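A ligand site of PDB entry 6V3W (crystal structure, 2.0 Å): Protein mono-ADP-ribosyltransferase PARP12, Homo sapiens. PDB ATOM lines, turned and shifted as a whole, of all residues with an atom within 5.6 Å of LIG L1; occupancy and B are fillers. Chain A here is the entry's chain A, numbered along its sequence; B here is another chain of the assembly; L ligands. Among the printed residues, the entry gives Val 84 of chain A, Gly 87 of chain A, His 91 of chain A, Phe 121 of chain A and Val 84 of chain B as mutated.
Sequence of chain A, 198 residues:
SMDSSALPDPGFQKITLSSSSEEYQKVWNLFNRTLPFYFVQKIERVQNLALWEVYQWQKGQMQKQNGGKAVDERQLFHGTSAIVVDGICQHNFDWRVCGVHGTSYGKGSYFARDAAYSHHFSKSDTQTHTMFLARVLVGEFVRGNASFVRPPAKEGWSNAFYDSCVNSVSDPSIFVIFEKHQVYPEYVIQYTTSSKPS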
ATOM      1  N   PHE A  77      11.909  23.514  -0.704  1.00  0.00           N
ATOM      2  CA  PHE A  77      12.745  24.311   0.208  1.00  0.00           C
ATOM      3  C   PHE A  77      13.665  23.367   0.982  1.00  0.00           C
ATOM      4  O   PHE A  77      13.273  22.215   1.273  1.00  0.00           O
ATOM      5  CB  PHE A  77      11.880  25.121   1.169  1.00  0.00           C
ATOM      6  CG  PHE A  77      11.140  26.202   0.443  1.00  0.00           C
ATOM      7  CD1 PHE A  77      11.768  27.402   0.133  1.00  0.00           C
ATOM      8  CD2 PHE A  77       9.831  26.007   0.032  1.00  0.00           C
ATOM      9  CE1 PHE A  77      11.079  28.415  -0.510  1.00  0.00           C
ATOM     10  CE2 PHE A  77       9.158  27.016  -0.636  1.00  0.00           C
ATOM     11  CZ  PHE A  77       9.773  28.226  -0.892  1.00  0.00           C
ATOM     12  N   HIS A  78      14.820  23.894   1.370  1.00  0.00           N
ATOM     13  CA  HIS A  78      15.724  23.250   2.352  1.00  0.00           C
ATOM     14  C   HIS A  78      16.381  24.345   3.227  1.00  0.00           C
ATOM     15  O   HIS A  78      17.207  25.118   2.695  1.00  0.00           O
ATOM     16  CB  HIS A  78      16.739  22.392   1.576  1.00  0.00           C
ATOM     17  CG  HIS A  78      17.569  21.567   2.470  1.00  0.00           C
ATOM     18  ND1 HIS A  78      17.213  20.315   2.832  1.00  0.00           N
ATOM     19  CD2 HIS A  78      18.707  21.860   3.147  1.00  0.00           C
ATOM     20  CE1 HIS A  78      18.064  19.860   3.730  1.00  0.00           C
ATOM     21  NE2 HIS A  78      19.003  20.782   3.922  1.00  0.00           N
ATOM     22  N   GLY A  79      16.034  24.392   4.502  1.00  0.00           N
ATOM     23  CA  GLY A  79      16.647  25.309   5.479  1.00  0.00           C
ATOM     24  C   GLY A  79      18.028  24.831   5.896  1.00  0.00           C
ATOM     25  O   GLY A  79      18.140  23.630   6.213  1.00  0.00           O
ATOM     26  N   THR A  80      19.037  25.710   5.883  1.00  0.00           N
ATOM     27  CA  THR A  80      20.461  25.385   6.216  1.00  0.00           C
ATOM     28  C   THR A  80      21.015  26.430   7.164  1.00  0.00           C
ATOM     29  O   THR A  80      20.276  27.343   7.501  1.00  0.00           O
ATOM     30  CB  THR A  80      21.372  25.368   4.983  1.00  0.00           C
ATOM     31  OG1 THR A  80      21.060  26.473   4.126  1.00  0.00           O
ATOM     32  CG2 THR A  80      21.257  24.103   4.165  1.00  0.00           C
ATOM     33  N   VAL A  84      27.270  26.509   5.413  1.00  0.00           N
ATOM     34  CA  VAL A  84      27.358  25.410   4.385  1.00  0.00           C
ATOM     35  C   VAL A  84      26.844  25.896   3.015  1.00  0.00           C
ATOM     36  O   VAL A  84      26.929  25.118   2.076  1.00  0.00           O
ATOM     37  CB  VAL A  84      26.608  24.124   4.777  1.00  0.00           C
ATOM     38  CG1 VAL A  84      27.144  23.522   6.054  1.00  0.00           C
ATOM     39  CG2 VAL A  84      25.097  24.296   4.864  1.00  0.00           C
ATOM     40  N   GLY A  87      29.237  25.540   0.220  1.00  0.00           N
ATOM     41  CA  GLY A  87      29.528  24.107   0.068  1.00  0.00           C
ATOM     42  C   GLY A  87      28.433  23.428  -0.751  1.00  0.00           C
ATOM     43  O   GLY A  87      28.751  22.706  -1.703  1.00  0.00           O
ATOM     44  N   ILE A  88      27.171  23.729  -0.450  1.00  0.00           N
ATOM     45  CA  ILE A  88      26.022  23.183  -1.232  1.00  0.00           C
ATOM     46  C   ILE A  88      26.029  23.789  -2.639  1.00  0.00           C
ATOM     47  O   ILE A  88      25.902  23.008  -3.598  1.00  0.00           O
ATOM     48  CB  ILE A  88      24.719  23.380  -0.457  1.00  0.00           C
ATOM     49  CG1 ILE A  88      24.715  22.457   0.764  1.00  0.00           C
ATOM     50  CG2 ILE A  88      23.495  23.183  -1.349  1.00  0.00           C
ATOM     51  CD1 ILE A  88      23.674  22.824   1.807  1.00  0.00           C
ATOM     52  N   HIS A  91      28.936  21.704  -4.298  1.00  0.00           N
ATOM     53  CA  HIS A  91      28.990  20.220  -4.188  1.00  0.00           C
ATOM     54  C   HIS A  91      27.591  19.600  -4.123  1.00  0.00           C
ATOM     55  O   HIS A  91      27.503  18.391  -4.110  1.00  0.00           O
ATOM     56  CB  HIS A  91      29.711  19.777  -2.894  1.00  0.00           C
ATOM     57  CG  HIS A  91      31.178  20.005  -2.843  1.00  0.00           C
ATOM     58  ND1 HIS A  91      32.093  19.119  -3.431  1.00  0.00           N
ATOM     59  CD2 HIS A  91      31.913  20.925  -2.190  1.00  0.00           C
ATOM     60  CE1 HIS A  91      33.334  19.516  -3.183  1.00  0.00           C
ATOM     61  NE2 HIS A  91      33.254  20.626  -2.428  1.00  0.00           N
ATOM     62  N   ASN A  92      26.538  20.396  -3.986  1.00  0.00           N
ATOM     63  CA  ASN A  92      25.136  19.915  -3.837  1.00  0.00           C
ATOM     64  C   ASN A  92      24.861  19.394  -2.421  1.00  0.00           C
ATOM     65  O   ASN A  92      25.796  19.228  -1.628  1.00  0.00           O
ATOM     66  CB  ASN A  92      24.820  18.801  -4.848  1.00  0.00           C
ATOM     67  CG  ASN A  92      23.405  18.879  -5.378  1.00  0.00           C
ATOM     68  OD1 ASN A  92      22.565  19.553  -4.793  1.00  0.00           O
ATOM     69  ND2 ASN A  92      23.135  18.158  -6.464  1.00  0.00           N
ATOM     70  N   PHE A  93      23.599  19.110  -2.162  1.00  0.00           N
ATOM     71  CA  PHE A  93      23.084  18.408  -0.970  1.00  0.00           C
ATOM     72  C   PHE A  93      23.637  16.980  -0.957  1.00  0.00           C
ATOM     73  O   PHE A  93      23.543  16.292  -1.970  1.00  0.00           O
ATOM     74  CB  PHE A  93      21.564  18.433  -0.999  1.00  0.00           C
ATOM     75  CG  PHE A  93      20.965  19.805  -1.058  1.00  0.00           C
ATOM     76  CD1 PHE A  93      20.784  20.547   0.101  1.00  0.00           C
ATOM     77  CD2 PHE A  93      20.622  20.384  -2.263  1.00  0.00           C
ATOM     78  CE1 PHE A  93      20.274  21.834   0.057  1.00  0.00           C
ATOM     79  CE2 PHE A  93      20.090  21.662  -2.303  1.00  0.00           C
ATOM     80  CZ  PHE A  93      19.943  22.392  -1.149  1.00  0.00           C
ATOM     81  N   ASP A  94      24.165  16.558   0.175  1.00  0.00           N
ATOM     82  CA  ASP A  94      24.621  15.171   0.424  1.00  0.00           C
ATOM     83  C   ASP A  94      24.238  14.842   1.861  1.00  0.00           C
ATOM     84  O   ASP A  94      24.836  15.418   2.793  1.00  0.00           O
ATOM     85  CB  ASP A  94      26.119  15.026   0.144  1.00  0.00           C
ATOM     86  CG  ASP A  94      26.541  13.632  -0.293  1.00  0.00           C
ATOM     87  OD1 ASP A  94      26.038  12.652   0.324  1.00  0.00           O
ATOM     88  OD2 ASP A  94      27.388  13.531  -1.239  1.00  0.00           O
ATOM     89  N   TRP A  95      23.222  13.993   2.029  1.00  0.00           N
ATOM     90  CA  TRP A  95      22.714  13.587   3.368  1.00  0.00           C
ATOM     91  C   TRP A  95      23.789  12.856   4.178  1.00  0.00           C
ATOM     92  O   TRP A  95      23.625  12.752   5.398  1.00  0.00           O
ATOM     93  CB  TRP A  95      21.475  12.697   3.218  1.00  0.00           C
ATOM     94  CG  TRP A  95      21.801  11.349   2.675  1.00  0.00           C
ATOM     95  CD1 TRP A  95      21.822  10.977   1.359  1.00  0.00           C
ATOM     96  CD2 TRP A  95      22.164  10.177   3.431  1.00  0.00           C
ATOM     97  NE1 TRP A  95      22.185   9.657   1.249  1.00  0.00           N
ATOM     98  CE2 TRP A  95      22.398   9.151   2.498  1.00  0.00           C
ATOM     99  CE3 TRP A  95      22.323   9.922   4.799  1.00  0.00           C
ATOM    100  CZ2 TRP A  95      22.758   7.859   2.899  1.00  0.00           C
ATOM    101  CZ3 TRP A  95      22.694   8.651   5.191  1.00  0.00           C
ATOM    102  CH2 TRP A  95      22.895   7.643   4.255  1.00  0.00           C
ATOM    103  N   VAL A  97      26.757  13.738   4.855  1.00  0.00           N
ATOM    104  CA  VAL A  97      27.505  14.712   5.707  1.00  0.00           C
ATOM    105  C   VAL A  97      27.009  14.544   7.154  1.00  0.00           C
ATOM    106  O   VAL A  97      27.877  14.454   8.027  1.00  0.00           O
ATOM    107  CB  VAL A  97      27.349  16.168   5.230  1.00  0.00           C
ATOM    108  CG1 VAL A  97      27.917  17.153   6.236  1.00  0.00           C
ATOM    109  CG2 VAL A  97      27.976  16.375   3.866  1.00  0.00           C
ATOM    110  N   CYS A  98      25.698  14.503   7.379  1.00  0.00           N
ATOM    111  CA  CYS A  98      25.087  14.540   8.732  1.00  0.00           C
ATOM    112  C   CYS A  98      24.561  13.178   9.177  1.00  0.00           C
ATOM    113  O   CYS A  98      24.647  12.892  10.378  1.00  0.00           O
ATOM    114  CB  CYS A  98      23.936  15.545   8.792  1.00  0.00           C
ATOM    115  SG  CYS A  98      24.482  17.276   8.781  1.00  0.00           S
ATOM    116  N   GLY A  99      24.005  12.384   8.257  1.00  0.00           N
ATOM    117  CA  GLY A  99      23.063  11.289   8.583  1.00  0.00           C
ATOM    118  C   GLY A  99      21.701  11.836   9.030  1.00  0.00           C
ATOM    119  O   GLY A  99      21.508  13.071   9.019  1.00  0.00           O
ATOM    120  N   VAL A 100      20.784  10.922   9.388  1.00  0.00           N
ATOM    121  CA  VAL A 100      19.414  11.196   9.912  1.00  0.00           C
ATOM    122  C   VAL A 100      19.229  10.347  11.172  1.00  0.00           C
ATOM    123  O   VAL A 100      19.548   9.143  11.111  1.00  0.00           O
ATOM    124  CB  VAL A 100      18.335  10.867   8.849  1.00  0.00           C
ATOM    125  CG1 VAL A 100      16.944  11.296   9.295  1.00  0.00           C
ATOM    126  CG2 VAL A 100      18.675  11.444   7.483  1.00  0.00           C
ATOM    127  N   GLY A 108      18.024   9.860   3.265  1.00  0.00           N
ATOM    128  CA  GLY A 108      18.205  10.700   2.072  1.00  0.00           C
ATOM    129  C   GLY A 108      18.236  12.154   2.481  1.00  0.00           C
ATOM    130  O   GLY A 108      18.124  12.427   3.653  1.00  0.00           O
ATOM    131  N   SER A 109      18.429  13.056   1.531  1.00  0.00           N
ATOM    132  CA  SER A 109      18.267  14.509   1.740  1.00  0.00           C
ATOM    133  C   SER A 109      16.771  14.810   1.748  1.00  0.00           C
ATOM    134  O   SER A 109      16.078  14.261   0.906  1.00  0.00           O
ATOM    135  CB  SER A 109      19.026  15.282   0.719  1.00  0.00           C
ATOM    136  OG  SER A 109      20.419  15.165   0.948  1.00  0.00           O
ATOM    137  N   TYR A 110      16.303  15.633   2.676  1.00  0.00           N
ATOM    138  CA  TYR A 110      14.893  16.075   2.783  1.00  0.00           C
ATOM    139  C   TYR A 110      14.689  17.467   2.181  1.00  0.00           C
ATOM    140  O   TYR A 110      15.498  18.380   2.409  1.00  0.00           O
ATOM    141  CB  TYR A 110      14.478  16.175   4.245  1.00  0.00           C
ATOM    142  CG  TYR A 110      14.269  14.805   4.841  1.00  0.00           C
ATOM    143  CD1 TYR A 110      15.246  13.826   4.676  1.00  0.00           C
ATOM    144  CD2 TYR A 110      13.109  14.471   5.509  1.00  0.00           C
ATOM    145  CE1 TYR A 110      15.065  12.557   5.186  1.00  0.00           C
ATOM    146  CE2 TYR A 110      12.923  13.212   6.039  1.00  0.00           C
ATOM    147  CZ  TYR A 110      13.901  12.244   5.857  1.00  0.00           C
ATOM    148  OH  TYR A 110      13.761  10.985   6.368  1.00  0.00           O
ATOM    149  N   PHE A 111      13.562  17.637   1.511  1.00  0.00           N
ATOM    150  CA  PHE A 111      13.076  18.896   0.946  1.00  0.00           C
ATOM    151  C   PHE A 111      11.609  19.052   1.313  1.00  0.00           C
ATOM    152  O   PHE A 111      10.897  18.041   1.399  1.00  0.00           O
ATOM    153  CB  PHE A 111      13.304  18.898  -0.557  1.00  0.00           C
ATOM    154  CG  PHE A 111      14.757  18.684  -0.879  1.00  0.00           C
ATOM    155  CD1 PHE A 111      15.266  17.405  -0.977  1.00  0.00           C
ATOM    156  CD2 PHE A 111      15.626  19.757  -0.961  1.00  0.00           C
ATOM    157  CE1 PHE A 111      16.611  17.205  -1.232  1.00  0.00           C
ATOM    158  CE2 PHE A 111      16.971  19.562  -1.224  1.00  0.00           C
ATOM    159  CZ  PHE A 111      17.457  18.284  -1.350  1.00  0.00           C
ATOM    160  N   ALA A 112      11.179  20.289   1.540  1.00  0.00           N
ATOM    161  CA  ALA A 112       9.805  20.581   1.978  1.00  0.00           C
ATOM    162  C   ALA A 112       9.101  21.420   0.928  1.00  0.00           C
ATOM    163  O   ALA A 112       9.746  22.301   0.274  1.00  0.00           O
ATOM    164  CB  ALA A 112       9.840  21.264   3.310  1.00  0.00           C
ATOM    165  N   TYR A 117       7.926  25.047   6.968  1.00  0.00           N
ATOM    166  CA  TYR A 117       8.456  23.782   7.523  1.00  0.00           C
ATOM    167  C   TYR A 117       9.989  23.800   7.473  1.00  0.00           C
ATOM    168  O   TYR A 117      10.612  23.444   8.468  1.00  0.00           O
ATOM    169  CB  TYR A 117       7.893  22.544   6.807  1.00  0.00           C
ATOM    170  CG  TYR A 117       8.277  21.277   7.511  1.00  0.00           C
ATOM    171  CD1 TYR A 117       7.741  20.957   8.747  1.00  0.00           C
ATOM    172  CD2 TYR A 117       9.233  20.443   6.989  1.00  0.00           C
ATOM    173  CE1 TYR A 117       8.137  19.817   9.431  1.00  0.00           C
ATOM    174  CE2 TYR A 117       9.637  19.290   7.641  1.00  0.00           C
ATOM    175  CZ  TYR A 117       9.092  18.989   8.864  1.00  0.00           C
ATOM    176  OH  TYR A 117       9.492  17.844   9.483  1.00  0.00           O
ATOM    177  N   SER A 118      10.593  24.191   6.358  1.00  0.00           N
ATOM    178  CA  SER A 118      12.080  24.235   6.271  1.00  0.00           C
ATOM    179  C   SER A 118      12.646  25.267   7.261  1.00  0.00           C
ATOM    180  O   SER A 118      13.801  25.130   7.650  1.00  0.00           O
ATOM    181  CB  SER A 118      12.542  24.525   4.867  1.00  0.00           C
ATOM    182  OG  SER A 118      12.329  23.411   4.043  1.00  0.00           O
ATOM    183  N   PHE A 121      14.716  24.332  10.346  1.00  0.00           N
ATOM    184  CA  PHE A 121      16.106  23.818  10.173  1.00  0.00           C
ATOM    185  C   PHE A 121      17.065  24.932   9.715  1.00  0.00           C
ATOM    186  O   PHE A 121      18.244  24.649   9.501  1.00  0.00           O
ATOM    187  CB  PHE A 121      16.105  22.621   9.223  1.00  0.00           C
ATOM    188  CG  PHE A 121      15.126  21.544   9.618  1.00  0.00           C
ATOM    189  CD1 PHE A 121      13.802  21.571   9.163  1.00  0.00           C
ATOM    190  CD2 PHE A 121      15.498  20.511  10.447  1.00  0.00           C
ATOM    191  CE1 PHE A 121      12.896  20.583   9.509  1.00  0.00           C
ATOM    192  CE2 PHE A 121      14.591  19.517  10.800  1.00  0.00           C
ATOM    193  CZ  PHE A 121      13.297  19.567  10.341  1.00  0.00           C
ATOM    194  N   ILE A 174       6.631  16.567   2.186  1.00  0.00           N
ATOM    195  CA  ILE A 174       8.078  16.305   2.432  1.00  0.00           C
ATOM    196  C   ILE A 174       8.542  15.247   1.450  1.00  0.00           C
ATOM    197  O   ILE A 174       7.837  14.248   1.262  1.00  0.00           O
ATOM    198  CB  ILE A 174       8.327  15.906   3.885  1.00  0.00           C
ATOM    199  CG1 ILE A 174       7.847  16.998   4.828  1.00  0.00           C
ATOM    200  CG2 ILE A 174       9.784  15.564   4.125  1.00  0.00           C
ATOM    201  CD1 ILE A 174       8.043  16.671   6.300  1.00  0.00           C
ATOM    202  N   ILE B  83      33.870  15.318   1.599  1.00  0.00           N
ATOM    203  CA  ILE B  83      33.252  16.490   0.930  1.00  0.00           C
ATOM    204  C   ILE B  83      33.234  17.704   1.866  1.00  0.00           C
ATOM    205  O   ILE B  83      33.195  18.794   1.320  1.00  0.00           O
ATOM    206  CB  ILE B  83      31.877  16.126   0.342  1.00  0.00           C
ATOM    207  CG1 ILE B  83      30.764  16.207   1.382  1.00  0.00           C
ATOM    208  CG2 ILE B  83      31.913  14.768  -0.372  1.00  0.00           C
ATOM    209  CD1 ILE B  83      29.506  16.787   0.822  1.00  0.00           C
ATOM    210  N   VAL B  84      33.327  17.567   3.197  1.00  0.00           N
ATOM    211  CA  VAL B  84      33.333  18.734   4.140  1.00  0.00           C
ATOM    212  C   VAL B  84      34.753  19.100   4.576  1.00  0.00           C
ATOM    213  O   VAL B  84      34.889  20.094   5.293  1.00  0.00           O
ATOM    214  CB  VAL B  84      32.454  18.511   5.394  1.00  0.00           C
ATOM    215  CG1 VAL B  84      31.011  18.277   5.047  1.00  0.00           C
ATOM    216  CG2 VAL B  84      32.979  17.424   6.306  1.00  0.00           C
ATOM    217  N   VAL B  97      25.694  22.753  12.047  1.00  0.00           N
ATOM    218  CA  VAL B  97      25.486  22.278  10.651  1.00  0.00           C
ATOM    219  C   VAL B  97      24.525  21.089  10.687  1.00  0.00           C
ATOM    220  O   VAL B  97      23.578  21.095   9.891  1.00  0.00           O
ATOM    221  CB  VAL B  97      26.803  21.901   9.949  1.00  0.00           C
ATOM    222  CG1 VAL B  97      26.556  21.210   8.604  1.00  0.00           C
ATOM    223  CG2 VAL B  97      27.701  23.114   9.760  1.00  0.00           C
HETATM  224  C1  LIG L   1      18.174  15.379   6.654  1.00  0.00           C
HETATM  225  C2  LIG L   1      19.562  15.992   6.410  1.00  0.00           C
HETATM  226  C3  LIG L   1      19.693  16.667   5.058  1.00  0.00           C
HETATM  227  C4  LIG L   1      21.908  17.523   5.706  1.00  0.00           C
HETATM  228  N1  LIG L   1      23.406  18.154   3.781  1.00  0.00           N
HETATM  229  C5  LIG L   1      22.338  17.762   2.836  1.00  0.00           C
HETATM  230  C6  LIG L   1      24.584  18.791   3.401  1.00  0.00           C
HETATM  231  C7  LIG L   1      26.108  19.254   1.719  1.00  0.00           C
HETATM  232  C8  LIG L   1      28.237  20.509   2.143  1.00  0.00           C
HETATM  233  C9  LIG L   1      15.307  19.069   6.874  1.00  0.00           C
HETATM  234  C10 LIG L   1      15.137  21.185   5.714  1.00  0.00           C
HETATM  235  C11 LIG L   1      14.127  16.309   9.061  1.00  0.00           C
HETATM  236  C12 LIG L   1      15.315  17.009   8.370  1.00  0.00           C
HETATM  237  C13 LIG L   1      16.233  15.883   7.885  1.00  0.00           C
HETATM  238  O1  LIG L   1      17.339  16.410   7.183  1.00  0.00           O
HETATM  239  O2  LIG L   1      18.797  16.575   4.262  1.00  0.00           O
HETATM  240  N2  LIG L   1      20.814  17.360   4.721  1.00  0.00           N
HETATM  241  C14 LIG L   1      23.312  17.658   5.154  1.00  0.00           C
HETATM  242  C15 LIG L   1      20.957  18.017   3.419  1.00  0.00           C
HETATM  243  N3  LIG L   1      24.974  18.699   2.138  1.00  0.00           N
HETATM  244  C16 LIG L   1      26.939  19.919   2.625  1.00  0.00           C
HETATM  245  C17 LIG L   1      26.536  19.968   3.966  1.00  0.00           C
HETATM  246  N4  LIG L   1      25.372  19.387   4.302  1.00  0.00           N
HETATM  247  F1  LIG L   1      28.724  21.443   3.028  1.00  0.00           F
HETATM  248  F2  LIG L   1      29.130  19.459   2.014  1.00  0.00           F
HETATM  249  F3  LIG L   1      28.170  21.104   0.890  1.00  0.00           F
HETATM  250  N5  LIG L   1      14.766  17.847   7.268  1.00  0.00           N
HETATM  251  C18 LIG L   1      14.571  19.963   6.080  1.00  0.00           C
HETATM  252  O3  LIG L   1      14.509  21.973   5.045  1.00  0.00           O
HETATM  253  N6  LIG L   1      16.390  21.479   6.101  1.00  0.00           N
HETATM  254  N7  LIG L   1      17.111  20.573   6.873  1.00  0.00           N
HETATM  255  C19 LIG L   1      16.605  19.430   7.253  1.00  0.00           C
HETATM  256  C20 LIG L   1      13.181  19.673   5.615  1.00  0.00           C
HETATM  257  F4  LIG L   1      12.792  18.415   5.992  1.00  0.00           F
HETATM  258  F5  LIG L   1      13.105  19.745   4.240  1.00  0.00           F
HETATM  259  F6  LIG L   1      12.303  20.602   6.152  1.00  0.00           F
HETATM  260  C1  LG2 L   2      28.152  15.399  16.478  1.00  0.00           C
HETATM  261  C2  LG2 L   2      28.287  16.208  15.184  1.00  0.00           C
HETATM  262  C3  LG2 L   2      29.634  16.909  15.033  1.00  0.00           C
HETATM  263  C4  LG2 L   2      29.040  17.547  12.738  1.00  0.00           C
HETATM  264  N1  LG2 L   2      30.322  19.518  11.833  1.00  0.00           N
HETATM  265  C5  LG2 L   2      31.064  19.599  13.103  1.00  0.00           C
HETATM  266  C6  LG2 L   2      30.638  20.260  10.690  1.00  0.00           C
HETATM  267  C7  LG2 L   2      31.628  22.150   9.796  1.00  0.00           C
HETATM  268  C8  LG2 L   2      31.481  22.733   7.367  1.00  0.00           C
HETATM  269  C9  LG2 L   2      31.262  11.938  16.023  1.00  0.00           C
HETATM  270  C10 LG2 L   2      33.486  11.735  15.093  1.00  0.00           C
HETATM  271  C11 LG2 L   2      28.326  10.859  18.017  1.00  0.00           C
HETATM  272  C12 LG2 L   2      28.896  11.788  16.931  1.00  0.00           C
HETATM  273  C13 LG2 L   2      28.225  13.147  17.160  1.00  0.00           C
HETATM  274  O1  LG2 L   2      28.705  14.103  16.239  1.00  0.00           O
HETATM  275  O2  LG2 L   2      30.412  16.887  15.953  1.00  0.00           O
HETATM  276  N2  LG2 L   2      29.960  17.557  13.886  1.00  0.00           N
HETATM  277  C14 LG2 L   2      29.068  18.763  11.824  1.00  0.00           C
HETATM  278  C15 LG2 L   2      31.249  18.232  13.733  1.00  0.00           C
HETATM  279  N3  LG2 L   2      31.340  21.374  10.834  1.00  0.00           N
HETATM  280  C16 LG2 L   2      31.170  21.821   8.528  1.00  0.00           C
HETATM  281  C17 LG2 L   2      30.386  20.676   8.399  1.00  0.00           C
HETATM  282  N4  LG2 L   2      30.134  19.941   9.483  1.00  0.00           N
HETATM  283  F1  LG2 L   2      31.298  22.096   6.169  1.00  0.00           F
HETATM  284  F2  LG2 L   2      30.613  23.814   7.459  1.00  0.00           F
HETATM  285  F3  LG2 L   2      32.757  23.281   7.382  1.00  0.00           F
HETATM  286  N5  LG2 L   2      30.370  11.822  17.093  1.00  0.00           N
HETATM  287  C18 LG2 L   2      32.610  11.624  16.181  1.00  0.00           C
HETATM  288  O3  LG2 L   2      34.654  11.451  15.210  1.00  0.00           O
HETATM  289  N6  LG2 L   2      33.021  12.158  13.909  1.00  0.00           N
HETATM  290  N7  LG2 L   2      31.665  12.492  13.776  1.00  0.00           N
HETATM  291  C19 LG2 L   2      30.823  12.370  14.763  1.00  0.00           C
HETATM  292  C20 LG2 L   2      33.191  11.143  17.477  1.00  0.00           C
HETATM  293  F4  LG2 L   2      32.241  11.166  18.463  1.00  0.00           F
HETATM  294  F5  LG2 L   2      34.220  11.966  17.870  1.00  0.00           F
HETATM  295  F6  LG2 L   2      33.681   9.854  17.332  1.00  0.00           F
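The backbone carbonyl oxygen (O) of Gly 87 sits close to a fluorine (F3) of LIG L1 (3.1 Å).
N of Ile 88 lies close to F3 of LIG L1, at 3.1 Å.
The backbone NH (N) of Phe 111 sits close to a fluorine (F5) of LIG L1, at 3.5 Å.
The backbone NH (N) of Ala 112 lies close to a fluorine (F5) of LIG L1 (3.4 Å).
O of Phe 77 touches F5 of LIG L1, at 3.9 Å.
Val 84 of chain A touches LIG L1 (CB to F1, 3.8 Å).
Asn 92 touches LIG L1 (O to C7, 3.4 Å).
Phe 93 touches LIG L1.
Trp 95 touches LIG L1.
Val 97 of chain A touches LIG L1.
Cys 98 touches LIG L1.
Ser 109 touches LIG L1.
Tyr 117 touches LIG L1 (CD2 to F6, 3.2 Å).
Phe 121 touches LIG L1 (CB to N7, 3.3 Å).
CD1 of Ile 83 of chain B touches F2 of LIG L1, at 2.9 Å.
Val 84 of chain B touches LIG L1.
Hydrophobic or aromatic side chains within 4 Å of LIG L1: His 78, Val 84 of chain A, Ile 88, Phe 93, Val 97 of chain A, Tyr 110, Ala 112, Tyr 117, Phe 121, Ile 83 of chain B and Val 84 of chain B.
Along chain A the residues within 4 Å of LIG L1 span positions 77 to 121.
The side-chain hydroxyl (OG) of Ser 118 sits at hydrogen-bond distance from the backbone carbonyl oxygen (O) of Phe 77, 3.2 Å away.
The backbone carbonyl oxygen (O) of Tyr 110 sits at hydrogen-bond distance from a ring nitrogen (ND1) of His 78, 2.6 Å away.
OG of Ser 109 lies within hydrogen-bond range of N of Trp 95.
The backbone carbonyl oxygen of Ala 112 sits at hydrogen-bond distance from the backbone NH of Phe 77, 2.7 Å away.
The backbone NH (N) of Gly 79 lies within hydrogen-bond range of an oxygen (O3) of LIG L1 (2.9 Å).
O of Gly 79 lies within hydrogen-bond range of N6 of LIG L1 (2.8 Å).
O3 of LIG L1 lies within hydrogen-bond range of OG of Ser 118.
A nitrogen (N3) of LIG L1 lies within hydrogen-bond range of the backbone NH (N) of Asp 94 (3.0 Å).
An oxygen (O2) of LIG L1 sits at hydrogen-bond distance from the backbone NH (N) of Tyr 110 (3.1 Å).
NE2 of His 78 lies close to N6 of LIG L1, at 3.5 Å.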
